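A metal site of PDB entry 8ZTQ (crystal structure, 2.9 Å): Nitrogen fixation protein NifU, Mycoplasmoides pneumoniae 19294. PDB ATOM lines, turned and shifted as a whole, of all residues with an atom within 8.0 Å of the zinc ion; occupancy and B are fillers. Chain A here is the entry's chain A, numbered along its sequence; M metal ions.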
ATOM      1  N   THR A  45      27.227  27.165   1.901  1.00  0.00           N
ATOM      2  CA  THR A  45      27.733  26.390   0.768  1.00  0.00           C
ATOM      3  C   THR A  45      27.136  26.946  -0.517  1.00  0.00           C
ATOM      4  O   THR A  45      26.025  27.486  -0.529  1.00  0.00           O
ATOM      5  CB  THR A  45      27.405  24.896   0.910  1.00  0.00           C
ATOM      6  OG1 THR A  45      28.244  24.145   0.025  1.00  0.00           O
ATOM      7  CG2 THR A  45      25.946  24.612   0.570  1.00  0.00           C
ATOM      8  N   SER A  47      26.912  24.919  -3.213  1.00  0.00           N
ATOM      9  CA  SER A  47      26.398  23.751  -3.914  1.00  0.00           C
ATOM     10  C   SER A  47      24.939  23.491  -3.619  1.00  0.00           C
ATOM     11  O   SER A  47      24.346  22.588  -4.230  1.00  0.00           O
ATOM     12  CB  SER A  47      27.238  22.526  -3.552  1.00  0.00           C
ATOM     13  OG  SER A  47      28.618  22.781  -3.756  1.00  0.00           O
ATOM     14  N   CYS A  48      24.339  24.229  -2.691  1.00  0.00           N
ATOM     15  CA  CYS A  48      22.942  24.076  -2.339  1.00  0.00           C
ATOM     16  C   CYS A  48      22.461  25.417  -1.768  1.00  0.00           C
ATOM     17  O   CYS A  48      23.125  26.442  -1.942  1.00  0.00           O
ATOM     18  CB  CYS A  48      22.750  22.920  -1.357  1.00  0.00           C
ATOM     19  SG  CYS A  48      21.042  22.362  -1.166  1.00  0.00           S
ATOM     20  N   ILE A  49      21.318  25.402  -1.098  1.00  0.00           N
ATOM     21  CA  ILE A  49      20.751  26.608  -0.491  1.00  0.00           C
ATOM     22  C   ILE A  49      21.075  26.629   0.994  1.00  0.00           C
ATOM     23  O   ILE A  49      20.418  27.340   1.767  1.00  0.00           O
ATOM     24  CB  ILE A  49      19.241  26.698  -0.721  1.00  0.00           C
ATOM     25  CG1 ILE A  49      18.607  25.311  -0.608  1.00  0.00           C
ATOM     26  CG2 ILE A  49      18.938  27.327  -2.069  1.00  0.00           C
ATOM     27  CD1 ILE A  49      18.112  24.985   0.786  1.00  0.00           C
ATOM     28  N   ASP A  50      22.074  25.857   1.404  1.00  0.00           N
ATOM     29  CA  ASP A  50      22.386  25.668   2.820  1.00  0.00           C
ATOM     30  C   ASP A  50      23.214  26.858   3.309  1.00  0.00           C
ATOM     31  O   ASP A  50      24.403  26.973   3.007  1.00  0.00           O
ATOM     32  CB  ASP A  50      23.129  24.357   3.034  1.00  0.00           C
ATOM     33  CG  ASP A  50      22.409  23.171   2.396  1.00  0.00           C
ATOM     34  OD1 ASP A  50      21.164  23.207   2.280  1.00  0.00           O
ATOM     35  OD2 ASP A  50      23.093  22.190   2.007  1.00  0.00           O
ATOM     36  N   ASN A  51      22.573  27.748   4.059  1.00  0.00           N
ATOM     37  CA  ASN A  51      23.247  28.858   4.740  1.00  0.00           C
ATOM     38  C   ASN A  51      22.680  28.906   6.153  1.00  0.00           C
ATOM     39  O   ASN A  51      21.567  29.408   6.367  1.00  0.00           O
ATOM     40  CB  ASN A  51      23.044  30.186   4.003  1.00  0.00           C
ATOM     41  CG  ASN A  51      23.840  31.319   4.621  1.00  0.00           C
ATOM     42  OD1 ASN A  51      24.838  31.079   5.296  1.00  0.00           O
ATOM     43  ND2 ASN A  51      23.397  32.553   4.400  1.00  0.00           N
ATOM     44  N   LEU A  52      23.429  28.381   7.105  1.00  0.00           N
ATOM     45  CA  LEU A  52      22.956  28.194   8.470  1.00  0.00           C
ATOM     46  C   LEU A  52      23.829  28.944   9.457  1.00  0.00           C
ATOM     47  O   LEU A  52      25.045  29.028   9.296  1.00  0.00           O
ATOM     48  CB  LEU A  52      22.931  26.705   8.832  1.00  0.00           C
ATOM     49  CG  LEU A  52      22.049  25.796   7.973  1.00  0.00           C
ATOM     50  CD1 LEU A  52      22.810  24.531   7.593  1.00  0.00           C
ATOM     51  CD2 LEU A  52      20.762  25.459   8.701  1.00  0.00           C
ATOM     52  N   ILE A  71      18.658  28.773   6.252  1.00  0.00           N
ATOM     53  CA  ILE A  71      18.149  27.962   5.153  1.00  0.00           C
ATOM     54  C   ILE A  71      18.973  26.686   5.063  1.00  0.00           C
ATOM     55  O   ILE A  71      20.177  26.693   5.348  1.00  0.00           O
ATOM     56  CB  ILE A  71      18.202  28.753   3.826  1.00  0.00           C
ATOM     57  CG1 ILE A  71      17.697  30.173   4.029  1.00  0.00           C
ATOM     58  CG2 ILE A  71      17.380  28.050   2.747  1.00  0.00           C
ATOM     59  CD1 ILE A  71      17.573  30.974   2.737  1.00  0.00           C
ATOM     60  N   GLY A  72      18.335  25.596   4.658  1.00  0.00           N
ATOM     61  CA  GLY A  72      19.046  24.335   4.540  1.00  0.00           C
ATOM     62  C   GLY A  72      18.169  23.268   3.950  1.00  0.00           C
ATOM     63  O   GLY A  72      16.933  23.344   3.997  1.00  0.00           O
ATOM     64  N   CYS A  73      18.823  22.248   3.392  1.00  0.00           N
ATOM     65  CA  CYS A  73      18.118  21.101   2.853  1.00  0.00           C
ATOM     66  C   CYS A  73      17.918  20.056   3.947  1.00  0.00           C
ATOM     67  O   CYS A  73      18.252  20.255   5.121  1.00  0.00           O
ATOM     68  CB  CYS A  73      18.897  20.521   1.670  1.00  0.00           C
ATOM     69  SG  CYS A  73      20.588  19.992   2.037  1.00  0.00           S
ATOM     70  N   ALA A  74      17.369  18.912   3.550  1.00  0.00           N
ATOM     71  CA  ALA A  74      17.138  17.828   4.504  1.00  0.00           C
ATOM     72  C   ALA A  74      18.454  17.290   5.047  1.00  0.00           C
ATOM     73  O   ALA A  74      18.555  16.981   6.244  1.00  0.00           O
ATOM     74  CB  ALA A  74      16.337  16.716   3.837  1.00  0.00           C
ATOM     75  N   ILE A  75      19.476  17.170   4.194  1.00  0.00           N
ATOM     76  CA  ILE A  75      20.772  16.672   4.645  1.00  0.00           C
ATOM     77  C   ILE A  75      21.440  17.663   5.580  1.00  0.00           C
ATOM     78  O   ILE A  75      22.174  17.268   6.496  1.00  0.00           O
ATOM     79  CB  ILE A  75      21.671  16.346   3.439  1.00  0.00           C
ATOM     80  CG1 ILE A  75      20.876  15.612   2.360  1.00  0.00           C
ATOM     81  CG2 ILE A  75      22.857  15.504   3.870  1.00  0.00           C
ATOM     82  CD1 ILE A  75      20.578  14.168   2.700  1.00  0.00           C
ATOM     83  N   SER A  76      21.191  18.957   5.381  1.00  0.00           N
ATOM     84  CA  SER A  76      21.788  19.962   6.246  1.00  0.00           C
ATOM     85  C   SER A  76      20.995  20.132   7.538  1.00  0.00           C
ATOM     86  O   SER A  76      21.574  20.277   8.620  1.00  0.00           O
ATOM     87  CB  SER A  76      21.905  21.303   5.517  1.00  0.00           C
ATOM     88  OG  SER A  76      20.640  21.729   5.046  1.00  0.00           O
ATOM     89  N   THR A  77      19.662  20.103   7.451  1.00  0.00           N
ATOM     90  CA  THR A  77      18.844  20.344   8.629  1.00  0.00           C
ATOM     91  C   THR A  77      18.783  19.111   9.534  1.00  0.00           C
ATOM     92  O   THR A  77      18.589  19.248  10.749  1.00  0.00           O
ATOM     93  CB  THR A  77      17.439  20.798   8.227  1.00  0.00           C
ATOM     94  OG1 THR A  77      17.537  21.788   7.189  1.00  0.00           O
ATOM     95  CG2 THR A  77      16.710  21.395   9.403  1.00  0.00           C
ATOM     96  N   ASN A 130      27.190  15.792  -4.771  1.00  0.00           N
ATOM     97  CA  ASN A 130      27.062  17.134  -4.200  1.00  0.00           C
ATOM     98  C   ASN A 130      26.176  17.169  -2.964  1.00  0.00           C
ATOM     99  O   ASN A 130      25.398  18.103  -2.780  1.00  0.00           O
ATOM    100  CB  ASN A 130      26.552  18.127  -5.253  1.00  0.00           C
ATOM    101  CG  ASN A 130      25.187  17.756  -5.791  1.00  0.00           C
ATOM    102  OD1 ASN A 130      25.064  17.126  -6.841  1.00  0.00           O
ATOM    103  ND2 ASN A 130      24.145  18.157  -5.074  1.00  0.00           N
ATOM    104  N   ARG A 131      26.282  16.146  -2.116  1.00  0.00           N
ATOM    105  CA  ARG A 131      25.612  16.110  -0.830  1.00  0.00           C
ATOM    106  C   ARG A 131      26.600  16.093   0.331  1.00  0.00           C
ATOM    107  O   ARG A 131      26.177  16.183   1.490  1.00  0.00           O
ATOM    108  CB  ARG A 131      24.683  14.898  -0.740  1.00  0.00           C
ATOM    109  CG  ARG A 131      23.462  14.949  -1.641  1.00  0.00           C
ATOM    110  CD  ARG A 131      22.491  15.995  -1.147  1.00  0.00           C
ATOM    111  NE  ARG A 131      21.158  15.813  -1.707  1.00  0.00           N
ATOM    112  CZ  ARG A 131      20.097  16.514  -1.310  1.00  0.00           C
ATOM    113  NH1 ARG A 131      20.223  17.444  -0.375  1.00  0.00           N
ATOM    114  NH2 ARG A 131      18.918  16.283  -1.869  1.00  0.00           N
ATOM    115  N   ILE A 132      27.899  16.002   0.051  1.00  0.00           N
ATOM    116  CA  ILE A 132      28.913  15.943   1.100  1.00  0.00           C
ATOM    117  C   ILE A 132      28.983  17.286   1.828  1.00  0.00           C
ATOM    118  O   ILE A 132      29.111  17.336   3.058  1.00  0.00           O
ATOM    119  CB  ILE A 132      30.281  15.546   0.511  1.00  0.00           C
ATOM    120  CG1 ILE A 132      30.108  14.398  -0.501  1.00  0.00           C
ATOM    121  CG2 ILE A 132      31.242  15.160   1.625  1.00  0.00           C
ATOM    122  CD1 ILE A 132      30.094  14.871  -1.946  1.00  0.00           C
ATOM    123  N   LYS A 133      28.945  18.385   1.072  1.00  0.00           N
ATOM    124  CA  LYS A 133      28.965  19.710   1.693  1.00  0.00           C
ATOM    125  C   LYS A 133      27.642  20.025   2.389  1.00  0.00           C
ATOM    126  O   LYS A 133      27.617  20.903   3.261  1.00  0.00           O
ATOM    127  CB  LYS A 133      29.265  20.769   0.641  1.00  0.00           C
ATOM    128  CG  LYS A 133      30.387  20.383  -0.323  1.00  0.00           C
ATOM    129  CD  LYS A 133      31.064  21.625  -0.881  1.00  0.00           C
ATOM    130  CE  LYS A 133      31.984  21.298  -2.051  1.00  0.00           C
ATOM    131  NZ  LYS A 133      31.295  21.478  -3.362  1.00  0.00           N
ATOM    132  N   CYS A 134      26.571  19.319   2.038  1.00  0.00           N
ATOM    133  CA  CYS A 134      25.298  19.502   2.720  1.00  0.00           C
ATOM    134  C   CYS A 134      25.296  18.869   4.103  1.00  0.00           C
ATOM    135  O   CYS A 134      24.606  19.362   5.011  1.00  0.00           O
ATOM    136  CB  CYS A 134      24.171  18.927   1.866  1.00  0.00           C
ATOM    137  SG  CYS A 134      24.059  19.674   0.221  1.00  0.00           S
ATOM    138  N   ALA A 135      26.074  17.807   4.294  1.00  0.00           N
ATOM    139  CA  ALA A 135      26.190  17.107   5.557  1.00  0.00           C
ATOM    140  C   ALA A 135      27.421  17.526   6.356  1.00  0.00           C
ATOM    141  O   ALA A 135      27.700  16.947   7.407  1.00  0.00           O
ATOM    142  CB  ALA A 135      26.222  15.592   5.326  1.00  0.00           C
ATOM    143  N   VAL A 137      28.116  21.224   6.336  1.00  0.00           N
ATOM    144  CA  VAL A 137      28.038  22.681   6.426  1.00  0.00           C
ATOM    145  C   VAL A 137      27.697  23.108   7.858  1.00  0.00           C
ATOM    146  O   VAL A 137      28.346  24.008   8.413  1.00  0.00           O
ATOM    147  CB  VAL A 137      27.030  23.240   5.410  1.00  0.00           C
ATOM    148  CG1 VAL A 137      25.668  22.543   5.517  1.00  0.00           C
ATOM    149  CG2 VAL A 137      26.891  24.741   5.549  1.00  0.00           C
HETATM  150 ZN    ZN M   1      22.091  21.145   0.724  1.00  0.00          ZN
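Four residues have an atom within 4 Å of the zinc ion: Cys 48, Asp 50, Cys 73 and Cys 134. The nearest printed residue that does not touch the zinc ion is Arg 131 (4.3 Å).
The side-chain hydroxyl (OG) of Ser 76 is in hydrogen-bond range of the side-chain carboxylate (OD1) of Asp 50, 3.2 Å away. The backbone NH (N) of Thr 45 lies within hydrogen-bond range of the backbone carbonyl oxygen (O) of Asp 50, at 3.0 Å. SG of Cys 73 lies close to NH1 of Arg 131. The backbone NH of Cys 73 lies within hydrogen-bond range of the side-chain hydroxyl of Ser 76, at 2.5 Å. N of Ile 75 sits close to SG of Cys 73, at 3.7 Å. The side-chain hydroxyl (OG1) of Thr 77 is in hydrogen-bond range of the backbone carbonyl oxygen (O) of Cys 73. The backbone carbonyl oxygen (O) of Cys 134 lies close to the backbone NH (N) of Ser 76, 3.5 Å away. SG of Cys 134 lies close to O of Asn 130, 3.6 Å away.
The zinc ion is bound by OD2 of Asp 50 (1.9 Å), SG of Cys 73 (2.3 Å), SG of Cys 48 (2.5 Å) and SG of Cys 134 (2.5 Å). Slightly farther from the zinc ion lies the side-chain carboxylate (OD1) of Asp 50 (2.7 Å).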
